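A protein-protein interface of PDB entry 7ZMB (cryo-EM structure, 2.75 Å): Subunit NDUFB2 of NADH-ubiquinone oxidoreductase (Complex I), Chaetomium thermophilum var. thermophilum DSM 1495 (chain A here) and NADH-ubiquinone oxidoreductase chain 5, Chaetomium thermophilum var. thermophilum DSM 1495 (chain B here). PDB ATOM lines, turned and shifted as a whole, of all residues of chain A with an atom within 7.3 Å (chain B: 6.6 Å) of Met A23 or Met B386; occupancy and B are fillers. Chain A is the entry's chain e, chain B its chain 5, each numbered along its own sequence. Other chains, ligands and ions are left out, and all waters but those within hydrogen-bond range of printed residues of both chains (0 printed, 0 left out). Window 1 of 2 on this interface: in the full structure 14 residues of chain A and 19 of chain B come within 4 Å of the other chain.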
ATOM      1  N   THR A  17     -19.280   2.279 -20.746  1.00  0.00           N
ATOM      2  CA  THR A  17     -19.482   2.082 -19.316  1.00  0.00           C
ATOM      3  C   THR A  17     -18.283   1.406 -18.669  1.00  0.00           C
ATOM      4  O   THR A  17     -17.962   1.699 -17.513  1.00  0.00           O
ATOM      5  CB  THR A  17     -20.747   1.263 -19.068  1.00  0.00           C
ATOM      6  OG1 THR A  17     -20.610  -0.028 -19.676  1.00  0.00           O
ATOM      7  CG2 THR A  17     -21.960   1.969 -19.653  1.00  0.00           C
ATOM      8  N   GLY A  18     -17.613   0.505 -19.391  1.00  0.00           N
ATOM      9  CA  GLY A  18     -16.475  -0.192 -18.812  1.00  0.00           C
ATOM     10  C   GLY A  18     -15.358   0.752 -18.416  1.00  0.00           C
ATOM     11  O   GLY A  18     -14.811   0.662 -17.314  1.00  0.00           O
ATOM     12  N   LEU A  19     -15.032   1.706 -19.239  1.00  0.00           N
ATOM     13  CA  LEU A  19     -14.024   2.721 -18.845  1.00  0.00           C
ATOM     14  C   LEU A  19     -14.685   3.608 -17.791  1.00  0.00           C
ATOM     15  O   LEU A  19     -14.004   4.021 -16.843  1.00  0.00           O
ATOM     16  CB  LEU A  19     -13.625   3.529 -20.078  1.00  0.00           C
ATOM     17  CG  LEU A  19     -12.868   2.749 -21.151  1.00  0.00           C
ATOM     18  CD1 LEU A  19     -12.709   3.582 -22.411  1.00  0.00           C
ATOM     19  CD2 LEU A  19     -11.513   2.294 -20.635  1.00  0.00           C
ATOM     20  N   GLY A  20     -15.990   3.921 -17.992  1.00  0.00           N
ATOM     21  CA  GLY A  20     -16.685   4.653 -16.953  1.00  0.00           C
ATOM     22  C   GLY A  20     -16.788   3.900 -15.645  1.00  0.00           C
ATOM     23  O   GLY A  20     -16.944   4.528 -14.593  1.00  0.00           O
ATOM     24  N   ALA A  21     -16.712   2.569 -15.688  1.00  0.00           N
ATOM     25  CA  ALA A  21     -16.682   1.768 -14.471  1.00  0.00           C
ATOM     26  C   ALA A  21     -15.282   1.688 -13.880  1.00  0.00           C
ATOM     27  O   ALA A  21     -15.129   1.661 -12.655  1.00  0.00           O
ATOM     28  CB  ALA A  21     -17.210   0.359 -14.748  1.00  0.00           C
ATOM     29  N   SER A  22     -14.255   1.635 -14.731  1.00  0.00           N
ATOM     30  CA  SER A  22     -12.886   1.709 -14.234  1.00  0.00           C
ATOM     31  C   SER A  22     -12.649   3.033 -13.526  1.00  0.00           C
ATOM     32  O   SER A  22     -12.083   3.075 -12.427  1.00  0.00           O
ATOM     33  CB  SER A  22     -11.901   1.522 -15.387  1.00  0.00           C
ATOM     34  OG  SER A  22     -12.038   2.557 -16.343  1.00  0.00           O
ATOM     35  N   MET A  23     -13.086   4.129 -14.139  1.00  0.00           N
ATOM     36  CA  MET A  23     -13.147   5.397 -13.437  1.00  0.00           C
ATOM     37  C   MET A  23     -14.338   5.385 -12.481  1.00  0.00           C
ATOM     38  O   MET A  23     -15.181   4.485 -12.516  1.00  0.00           O
ATOM     39  CB  MET A  23     -13.253   6.555 -14.431  1.00  0.00           C
ATOM     40  CG  MET A  23     -12.824   7.904 -13.879  1.00  0.00           C
ATOM     41  SD  MET A  23     -13.399   9.268 -14.901  1.00  0.00           S
ATOM     42  CE  MET A  23     -15.006   9.571 -14.178  1.00  0.00           C
ATOM     43  N   TRP A  24     -14.376   6.375 -11.590  1.00  0.00           N
ATOM     44  CA  TRP A  24     -15.351   6.512 -10.511  1.00  0.00           C
ATOM     45  C   TRP A  24     -15.214   5.404  -9.477  1.00  0.00           C
ATOM     46  O   TRP A  24     -15.900   5.444  -8.449  1.00  0.00           O
ATOM     47  CB  TRP A  24     -16.801   6.541 -11.018  1.00  0.00           C
ATOM     48  CG  TRP A  24     -17.230   7.856 -11.591  1.00  0.00           C
ATOM     49  CD1 TRP A  24     -17.815   8.062 -12.804  1.00  0.00           C
ATOM     50  CD2 TRP A  24     -17.118   9.144 -10.976  1.00  0.00           C
ATOM     51  NE1 TRP A  24     -18.071   9.398 -12.986  1.00  0.00           N
ATOM     52  CE2 TRP A  24     -17.651  10.083 -11.876  1.00  0.00           C
ATOM     53  CE3 TRP A  24     -16.617   9.594  -9.751  1.00  0.00           C
ATOM     54  CZ2 TRP A  24     -17.698  11.444 -11.594  1.00  0.00           C
ATOM     55  CZ3 TRP A  24     -16.664  10.944  -9.472  1.00  0.00           C
ATOM     56  CH2 TRP A  24     -17.201  11.855 -10.389  1.00  0.00           C
ATOM     57  N   PHE A  25     -14.351   4.420  -9.712  1.00  0.00           N
ATOM     58  CA  PHE A  25     -13.965   3.431  -8.720  1.00  0.00           C
ATOM     59  C   PHE A  25     -12.533   3.608  -8.259  1.00  0.00           C
ATOM     60  O   PHE A  25     -12.222   3.303  -7.108  1.00  0.00           O
ATOM     61  CB  PHE A  25     -14.140   2.014  -9.280  1.00  0.00           C
ATOM     62  CG  PHE A  25     -13.635   0.931  -8.370  1.00  0.00           C
ATOM     63  CD1 PHE A  25     -14.403   0.484  -7.309  1.00  0.00           C
ATOM     64  CD2 PHE A  25     -12.394   0.352  -8.581  1.00  0.00           C
ATOM     65  CE1 PHE A  25     -13.940  -0.514  -6.472  1.00  0.00           C
ATOM     66  CE2 PHE A  25     -11.926  -0.645  -7.748  1.00  0.00           C
ATOM     67  CZ  PHE A  25     -12.700  -1.079  -6.692  1.00  0.00           C
ATOM     68  N   TRP A  26     -11.661   4.106  -9.137  1.00  0.00           N
ATOM     69  CA  TRP A  26     -10.301   4.441  -8.747  1.00  0.00           C
ATOM     70  C   TRP A  26     -10.258   5.600  -7.762  1.00  0.00           C
ATOM     71  O   TRP A  26      -9.274   5.738  -7.029  1.00  0.00           O
ATOM     72  CB  TRP A  26      -9.478   4.781  -9.990  1.00  0.00           C
ATOM     73  CG  TRP A  26      -8.076   5.195  -9.695  1.00  0.00           C
ATOM     74  CD1 TRP A  26      -7.591   6.467  -9.649  1.00  0.00           C
ATOM     75  CD2 TRP A  26      -6.972   4.333  -9.409  1.00  0.00           C
ATOM     76  NE1 TRP A  26      -6.252   6.451  -9.349  1.00  0.00           N
ATOM     77  CE2 TRP A  26      -5.848   5.152  -9.197  1.00  0.00           C
ATOM     78  CE3 TRP A  26      -6.825   2.946  -9.309  1.00  0.00           C
ATOM     79  CZ2 TRP A  26      -4.594   4.631  -8.892  1.00  0.00           C
ATOM     80  CZ3 TRP A  26      -5.580   2.433  -9.008  1.00  0.00           C
ATOM     81  CH2 TRP A  26      -4.481   3.272  -8.804  1.00  0.00           C
ATOM     82  N   ILE A  27     -11.301   6.426  -7.718  1.00  0.00           N
ATOM     83  CA  ILE A  27     -11.309   7.574  -6.817  1.00  0.00           C
ATOM     84  C   ILE A  27     -11.631   7.140  -5.393  1.00  0.00           C
ATOM     85  O   ILE A  27     -10.843   7.359  -4.466  1.00  0.00           O
ATOM     86  CB  ILE A  27     -12.300   8.641  -7.313  1.00  0.00           C
ATOM     87  CG1 ILE A  27     -11.919   9.104  -8.719  1.00  0.00           C
ATOM     88  CG2 ILE A  27     -12.335   9.818  -6.357  1.00  0.00           C
ATOM     89  CD1 ILE A  27     -13.069   9.702  -9.489  1.00  0.00           C
ATOM     90  N   SER B 371     -17.669   9.357 -22.883  1.00  0.00           N
ATOM     91  CA  SER B 371     -17.028   8.807 -21.695  1.00  0.00           C
ATOM     92  C   SER B 371     -15.554   9.176 -21.636  1.00  0.00           C
ATOM     93  O   SER B 371     -15.042   9.538 -20.572  1.00  0.00           O
ATOM     94  CB  SER B 371     -17.201   7.291 -21.659  1.00  0.00           C
ATOM     95  OG  SER B 371     -16.436   6.721 -20.614  1.00  0.00           O
ATOM     96  N   LEU B 374     -14.927  13.042 -20.995  1.00  0.00           N
ATOM     97  CA  LEU B 374     -15.095  13.332 -19.577  1.00  0.00           C
ATOM     98  C   LEU B 374     -13.872  12.889 -18.785  1.00  0.00           C
ATOM     99  O   LEU B 374     -13.381  13.623 -17.920  1.00  0.00           O
ATOM    100  CB  LEU B 374     -16.359  12.651 -19.055  1.00  0.00           C
ATOM    101  CG  LEU B 374     -16.848  13.003 -17.650  1.00  0.00           C
ATOM    102  CD1 LEU B 374     -18.360  12.906 -17.595  1.00  0.00           C
ATOM    103  CD2 LEU B 374     -16.232  12.083 -16.610  1.00  0.00           C
ATOM    104  N   ILE B 375     -13.362  11.692 -19.076  1.00  0.00           N
ATOM    105  CA  ILE B 375     -12.168  11.204 -18.393  1.00  0.00           C
ATOM    106  C   ILE B 375     -11.005  12.156 -18.623  1.00  0.00           C
ATOM    107  O   ILE B 375     -10.260  12.489 -17.693  1.00  0.00           O
ATOM    108  CB  ILE B 375     -11.829   9.779 -18.866  1.00  0.00           C
ATOM    109  CG1 ILE B 375     -12.894   8.790 -18.400  1.00  0.00           C
ATOM    110  CG2 ILE B 375     -10.458   9.367 -18.370  1.00  0.00           C
ATOM    111  CD1 ILE B 375     -12.823   7.455 -19.092  1.00  0.00           C
ATOM    112  N   ALA B 376     -10.833  12.607 -19.863  1.00  0.00           N
ATOM    113  CA  ALA B 376      -9.738  13.517 -20.171  1.00  0.00           C
ATOM    114  C   ALA B 376      -9.936  14.871 -19.507  1.00  0.00           C
ATOM    115  O   ALA B 376      -8.993  15.434 -18.942  1.00  0.00           O
ATOM    116  CB  ALA B 376      -9.609  13.678 -21.679  1.00  0.00           C
ATOM    117  N   LEU B 378     -11.583  15.617 -16.808  1.00  0.00           N
ATOM    118  CA  LEU B 378     -11.392  15.539 -15.364  1.00  0.00           C
ATOM    119  C   LEU B 378      -9.916  15.632 -15.003  1.00  0.00           C
ATOM    120  O   LEU B 378      -9.542  16.330 -14.053  1.00  0.00           O
ATOM    121  CB  LEU B 378     -12.004  14.251 -14.819  1.00  0.00           C
ATOM    122  CG  LEU B 378     -13.522  14.273 -14.640  1.00  0.00           C
ATOM    123  CD1 LEU B 378     -13.983  13.060 -13.856  1.00  0.00           C
ATOM    124  CD2 LEU B 378     -13.966  15.555 -13.955  1.00  0.00           C
ATOM    125  N   SER B 379      -9.060  14.938 -15.753  1.00  0.00           N
ATOM    126  CA  SER B 379      -7.624  15.104 -15.561  1.00  0.00           C
ATOM    127  C   SER B 379      -7.156  16.482 -16.009  1.00  0.00           C
ATOM    128  O   SER B 379      -6.184  17.011 -15.464  1.00  0.00           O
ATOM    129  CB  SER B 379      -6.872  14.004 -16.305  1.00  0.00           C
ATOM    130  OG  SER B 379      -7.122  14.084 -17.693  1.00  0.00           O
ATOM    131  N   LEU B 380      -7.829  17.075 -16.993  1.00  0.00           N
ATOM    132  CA  LEU B 380      -7.473  18.422 -17.414  1.00  0.00           C
ATOM    133  C   LEU B 380      -7.799  19.443 -16.334  1.00  0.00           C
ATOM    134  O   LEU B 380      -6.999  20.346 -16.062  1.00  0.00           O
ATOM    135  CB  LEU B 380      -8.189  18.771 -18.716  1.00  0.00           C
ATOM    136  CG  LEU B 380      -8.023  20.218 -19.186  1.00  0.00           C
ATOM    137  CD1 LEU B 380      -6.637  20.424 -19.761  1.00  0.00           C
ATOM    138  CD2 LEU B 380      -9.089  20.583 -20.204  1.00  0.00           C
ATOM    139  N   ALA B 382      -7.878  18.881 -13.282  1.00  0.00           N
ATOM    140  CA  ALA B 382      -7.206  18.439 -12.060  1.00  0.00           C
ATOM    141  C   ALA B 382      -8.213  17.960 -11.017  1.00  0.00           C
ATOM    142  O   ALA B 382      -8.153  18.328  -9.842  1.00  0.00           O
ATOM    143  CB  ALA B 382      -6.301  19.537 -11.494  1.00  0.00           C
ATOM    144  N   PHE B 383      -9.156  17.138 -11.464  1.00  0.00           N
ATOM    145  CA  PHE B 383     -10.007  16.419 -10.532  1.00  0.00           C
ATOM    146  C   PHE B 383      -9.136  15.509  -9.670  1.00  0.00           C
ATOM    147  O   PHE B 383      -8.226  14.855 -10.190  1.00  0.00           O
ATOM    148  CB  PHE B 383     -11.051  15.596 -11.290  1.00  0.00           C
ATOM    149  CG  PHE B 383     -12.195  15.132 -10.439  1.00  0.00           C
ATOM    150  CD1 PHE B 383     -13.205  16.005 -10.078  1.00  0.00           C
ATOM    151  CD2 PHE B 383     -12.260  13.822 -10.000  1.00  0.00           C
ATOM    152  CE1 PHE B 383     -14.257  15.581  -9.294  1.00  0.00           C
ATOM    153  CE2 PHE B 383     -13.310  13.392  -9.216  1.00  0.00           C
ATOM    154  CZ  PHE B 383     -14.309  14.273  -8.863  1.00  0.00           C
ATOM    155  N   PRO B 384      -9.374  15.448  -8.360  1.00  0.00           N
ATOM    156  CA  PRO B 384      -8.432  14.753  -7.477  1.00  0.00           C
ATOM    157  C   PRO B 384      -8.275  13.283  -7.833  1.00  0.00           C
ATOM    158  O   PRO B 384      -9.222  12.613  -8.252  1.00  0.00           O
ATOM    159  CB  PRO B 384      -9.050  14.934  -6.089  1.00  0.00           C
ATOM    160  CG  PRO B 384     -10.500  15.092  -6.346  1.00  0.00           C
ATOM    161  CD  PRO B 384     -10.607  15.832  -7.651  1.00  0.00           C
ATOM    162  N   PHE B 385      -7.042  12.799  -7.676  1.00  0.00           N
ATOM    163  CA  PHE B 385      -6.687  11.398  -7.903  1.00  0.00           C
ATOM    164  C   PHE B 385      -6.890  11.002  -9.365  1.00  0.00           C
ATOM    165  O   PHE B 385      -7.560  10.018  -9.683  1.00  0.00           O
ATOM    166  CB  PHE B 385      -7.467  10.479  -6.962  1.00  0.00           C
ATOM    167  CG  PHE B 385      -7.336  10.852  -5.518  1.00  0.00           C
ATOM    168  CD1 PHE B 385      -6.134  10.687  -4.855  1.00  0.00           C
ATOM    169  CD2 PHE B 385      -8.413  11.373  -4.824  1.00  0.00           C
ATOM    170  CE1 PHE B 385      -6.009  11.031  -3.524  1.00  0.00           C
ATOM    171  CE2 PHE B 385      -8.294  11.720  -3.494  1.00  0.00           C
ATOM    172  CZ  PHE B 385      -7.091  11.548  -2.843  1.00  0.00           C
ATOM    173  N   MET B 386      -6.299  11.787 -10.260  1.00  0.00           N
ATOM    174  CA  MET B 386      -6.282  11.498 -11.685  1.00  0.00           C
ATOM    175  C   MET B 386      -4.870  11.694 -12.217  1.00  0.00           C
ATOM    176  O   MET B 386      -3.952  12.077 -11.487  1.00  0.00           O
ATOM    177  CB  MET B 386      -7.268  12.387 -12.453  1.00  0.00           C
ATOM    178  CG  MET B 386      -8.718  12.166 -12.080  1.00  0.00           C
ATOM    179  SD  MET B 386      -9.305  10.555 -12.624  1.00  0.00           S
ATOM    180  CE  MET B 386     -10.517  11.044 -13.843  1.00  0.00           C
ATOM    181  N   THR B 387      -4.702  11.419 -13.513  1.00  0.00           N
ATOM    182  CA  THR B 387      -3.398  11.614 -14.140  1.00  0.00           C
ATOM    183  C   THR B 387      -2.989  13.080 -14.110  1.00  0.00           C
ATOM    184  O   THR B 387      -1.837  13.403 -13.805  1.00  0.00           O
ATOM    185  CB  THR B 387      -3.418  11.091 -15.577  1.00  0.00           C
ATOM    186  OG1 THR B 387      -3.444   9.659 -15.564  1.00  0.00           O
ATOM    187  CG2 THR B 387      -2.190  11.569 -16.344  1.00  0.00           C
ATOM    188  N   GLY B 388      -3.918  13.979 -14.410  1.00  0.00           N
ATOM    189  CA  GLY B 388      -3.614  15.394 -14.359  1.00  0.00           C
ATOM    190  C   GLY B 388      -3.629  16.008 -12.979  1.00  0.00           C
ATOM    191  O   GLY B 388      -3.135  17.126 -12.812  1.00  0.00           O
ATOM    192  N   PHE B 389      -4.184  15.305 -11.988  1.00  0.00           N
ATOM    193  CA  PHE B 389      -4.281  15.865 -10.643  1.00  0.00           C
ATOM    194  C   PHE B 389      -2.903  16.104 -10.042  1.00  0.00           C
ATOM    195  O   PHE B 389      -2.591  17.212  -9.598  1.00  0.00           O
ATOM    196  CB  PHE B 389      -5.098  14.934  -9.747  1.00  0.00           C
ATOM    197  CG  PHE B 389      -4.857  15.142  -8.280  1.00  0.00           C
ATOM    198  CD1 PHE B 389      -5.291  16.296  -7.650  1.00  0.00           C
ATOM    199  CD2 PHE B 389      -4.196  14.186  -7.529  1.00  0.00           C
ATOM    200  CE1 PHE B 389      -5.074  16.488  -6.301  1.00  0.00           C
ATOM    201  CE2 PHE B 389      -3.976  14.374  -6.180  1.00  0.00           C
ATOM    202  CZ  PHE B 389      -4.415  15.527  -5.565  1.00  0.00           C
ATOM    203  N   TYR B 390      -2.099  15.046  -9.987  1.00  0.00           N
ATOM    204  CA  TYR B 390      -0.764  15.195  -9.367  1.00  0.00           C
ATOM    205  C   TYR B 390       0.001  16.242 -10.177  1.00  0.00           C
ATOM    206  O   TYR B 390       0.580  17.156  -9.573  1.00  0.00           O
ATOM    207  CB  TYR B 390      -0.050  13.842  -9.307  1.00  0.00           C
ATOM    208  CG  TYR B 390      -0.815  12.755  -8.596  1.00  0.00           C
ATOM    209  CD1 TYR B 390      -0.738  12.607  -7.222  1.00  0.00           C
ATOM    210  CD2 TYR B 390      -1.616  11.868  -9.297  1.00  0.00           C
ATOM    211  CE1 TYR B 390      -1.438  11.611  -6.562  1.00  0.00           C
ATOM    212  CE2 TYR B 390      -2.327  10.871  -8.652  1.00  0.00           C
ATOM    213  CZ  TYR B 390      -2.237  10.739  -7.279  1.00  0.00           C
ATOM    214  OH  TYR B 390      -2.931   9.756  -6.636  1.00  0.00           O
ATOM    215  N   SER B 391      -0.006  16.112 -11.506  1.00  0.00           N
ATOM    216  CA  SER B 391       0.805  17.027 -12.350  1.00  0.00           C
ATOM    217  C   SER B 391       0.320  18.483 -12.334  1.00  0.00           C
ATOM    218  O   SER B 391       1.156  19.368 -12.090  1.00  0.00           O
ATOM    219  CB  SER B 391       0.830  16.494 -13.751  1.00  0.00           C
ATOM    220  OG  SER B 391      -0.477  16.426 -14.294  1.00  0.00           O
ATOM    221  N   PHE B 480      -4.486   5.585 -19.550  1.00  0.00           N
ATOM    222  CA  PHE B 480      -3.390   6.430 -19.083  1.00  0.00           C
ATOM    223  C   PHE B 480      -3.914   7.666 -18.366  1.00  0.00           C
ATOM    224  O   PHE B 480      -3.381   8.064 -17.325  1.00  0.00           O
ATOM    225  CB  PHE B 480      -2.495   6.829 -20.254  1.00  0.00           C
ATOM    226  CG  PHE B 480      -1.721   5.687 -20.846  1.00  0.00           C
ATOM    227  CD1 PHE B 480      -1.603   4.485 -20.170  1.00  0.00           C
ATOM    228  CD2 PHE B 480      -1.107   5.818 -22.077  1.00  0.00           C
ATOM    229  CE1 PHE B 480      -0.890   3.435 -20.714  1.00  0.00           C
ATOM    230  CE2 PHE B 480      -0.394   4.773 -22.625  1.00  0.00           C
ATOM    231  CZ  PHE B 480      -0.285   3.581 -21.944  1.00  0.00           C
ATOM    232  N   SER B 481      -4.970   8.278 -18.898  1.00  0.00           N
ATOM    233  CA  SER B 481      -5.513   9.483 -18.289  1.00  0.00           C
ATOM    234  C   SER B 481      -6.140   9.223 -16.926  1.00  0.00           C
ATOM    235  O   SER B 481      -6.457  10.185 -16.218  1.00  0.00           O
ATOM    236  CB  SER B 481      -6.539  10.120 -19.226  1.00  0.00           C
ATOM    237  OG  SER B 481      -7.373   9.137 -19.806  1.00  0.00           O
ATOM    238  N   ILE B 482      -6.329   7.966 -16.546  1.00  0.00           N
ATOM    239  CA  ILE B 482      -6.850   7.611 -15.232  1.00  0.00           C
ATOM    240  C   ILE B 482      -5.732   7.239 -14.268  1.00  0.00           C
ATOM    241  O   ILE B 482      -5.653   7.771 -13.164  1.00  0.00           O
ATOM    242  CB  ILE B 482      -7.879   6.466 -15.352  1.00  0.00           C
ATOM    243  CG1 ILE B 482      -9.124   6.929 -16.100  1.00  0.00           C
ATOM    244  CG2 ILE B 482      -8.266   5.954 -13.979  1.00  0.00           C
ATOM    245  CD1 ILE B 482     -10.084   5.813 -16.407  1.00  0.00           C
ATOM    246  N   PHE B 483      -4.849   6.328 -14.675  1.00  0.00           N
ATOM    247  CA  PHE B 483      -3.903   5.711 -13.756  1.00  0.00           C
ATOM    248  C   PHE B 483      -2.468   6.182 -13.909  1.00  0.00           C
ATOM    249  O   PHE B 483      -1.716   6.126 -12.935  1.00  0.00           O
ATOM    250  CB  PHE B 483      -3.922   4.185 -13.916  1.00  0.00           C
ATOM    251  CG  PHE B 483      -5.295   3.584 -13.889  1.00  0.00           C
ATOM    252  CD1 PHE B 483      -5.947   3.368 -12.690  1.00  0.00           C
ATOM    253  CD2 PHE B 483      -5.927   3.223 -15.064  1.00  0.00           C
ATOM    254  CE1 PHE B 483      -7.208   2.808 -12.665  1.00  0.00           C
ATOM    255  CE2 PHE B 483      -7.188   2.663 -15.045  1.00  0.00           C
ATOM    256  CZ  PHE B 483      -7.829   2.456 -13.845  1.00  0.00           C
ATOM    257  N   PHE B 484      -2.064   6.636 -15.098  1.00  0.00           N
ATOM    258  CA  PHE B 484      -0.647   6.891 -15.348  1.00  0.00           C
ATOM    259  C   PHE B 484      -0.080   7.946 -14.406  1.00  0.00           C
ATOM    260  O   PHE B 484       1.121   7.935 -14.117  1.00  0.00           O
ATOM    261  CB  PHE B 484      -0.437   7.309 -16.804  1.00  0.00           C
ATOM    262  CG  PHE B 484       1.004   7.501 -17.181  1.00  0.00           C
ATOM    263  CD1 PHE B 484       1.793   6.418 -17.528  1.00  0.00           C
ATOM    264  CD2 PHE B 484       1.567   8.764 -17.200  1.00  0.00           C
ATOM    265  CE1 PHE B 484       3.117   6.593 -17.878  1.00  0.00           C
ATOM    266  CE2 PHE B 484       2.890   8.944 -17.550  1.00  0.00           C
ATOM    267  CZ  PHE B 484       3.666   7.857 -17.889  1.00  0.00           C
ATOM    268  N   GLY B 485      -0.918   8.862 -13.921  1.00  0.00           N
ATOM    269  CA  GLY B 485      -0.431   9.870 -12.994  1.00  0.00           C
ATOM    270  C   GLY B 485       0.041   9.277 -11.680  1.00  0.00           C
ATOM    271  O   GLY B 485       1.123   9.605 -11.189  1.00  0.00           O
ATOM    272  N   PHE B 486      -0.759   8.383 -11.099  1.00  0.00           N
ATOM    273  CA  PHE B 486      -0.412   7.834  -9.793  1.00  0.00           C
ATOM    274  C   PHE B 486       0.791   6.905  -9.878  1.00  0.00           C
ATOM    275  O   PHE B 486       1.617   6.868  -8.960  1.00  0.00           O
ATOM    276  CB  PHE B 486      -1.605   7.095  -9.187  1.00  0.00           C
ATOM    277  CG  PHE B 486      -1.247   6.262  -7.994  1.00  0.00           C
ATOM    278  CD1 PHE B 486      -1.117   6.843  -6.745  1.00  0.00           C
ATOM    279  CD2 PHE B 486      -1.007   4.904  -8.125  1.00  0.00           C
ATOM    280  CE1 PHE B 486      -0.775   6.083  -5.646  1.00  0.00           C
ATOM    281  CE2 PHE B 486      -0.657   4.141  -7.031  1.00  0.00           C
ATOM    282  CZ  PHE B 486      -0.543   4.732  -5.788  1.00  0.00           C
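Of chain B, only Leu B374 (3.7 Å), Ile B375 (3.6 Å), Leu B378 (3.7 Å), Met B386 (3.5 Å) and Ile B482 (3.8 Å) come within 4 Å of Met A23. Of the printed residues of chain A, Met B386 touches Met A23. Of the printed residues of chain A, Ile B482 touches Ser A22 and Met A23. Of the printed residues of chain A, Ile B375 touches Met A23 (3.6 Å). Printed residues of chain A within 4 Å of Leu B378: Met A23 (3.7 Å). Printed residues of chain A within 4 Å of Leu B374: Met A23 (3.7 Å). Of the printed residues of chain B, Ile A27 touches Phe B383. The nearest residue of chain A that does not touch Met B386 is Ile A27 (4.9 Å).
N of Gly A20 touches OG of Ser B371, 3.9 Å away. CD1 of Ile B482 touches OG of Ser A22 (3.8 Å). Leu B374 touches Met A23 (CD2 to CE, 3.7 Å). Met A23 touches Ile B375. Met B386 touches Met A23. Met A23 touches Ile B482. CD1 of Trp A26 touches O of Phe B385, at 3.6 Å. CE3 of Trp A26 touches CE1 of Phe B483 (3.4 Å). Trp A26 touches Phe B486 (CZ2 to CD2, 3.7 Å). Ile A27 touches Phe B383.
The backbone carbonyl oxygen (O) of Leu B378 lies within hydrogen-bond range of the backbone NH (N) of Phe B383 (2.7 Å). The side-chain hydroxyl of Ser A22 lies within hydrogen-bond range of the backbone carbonyl oxygen of Gly A18 (3.5 Å). The backbone NH of Ile B482 is in hydrogen-bond range of the side-chain hydroxyl of Thr B387 (3.5 Å). The backbone carbonyl oxygen of Leu A19 lies within hydrogen-bond range of the side-chain hydroxyl of Ser A22, at 2.5 Å.
Printed residues of chain B that touch a printed residue of chain A: Ser B371, Leu B374, Ile B375, Leu B378, Phe B383, Phe B385, Met B386, Ile B482, Phe B483 and Phe B486. Among the printed residues, 11 pairs touch across the chains. Among the printed residues, no Asp or Glu carboxylate lies within 4 Å of a Lys or Arg side-chain nitrogen of the other chain.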
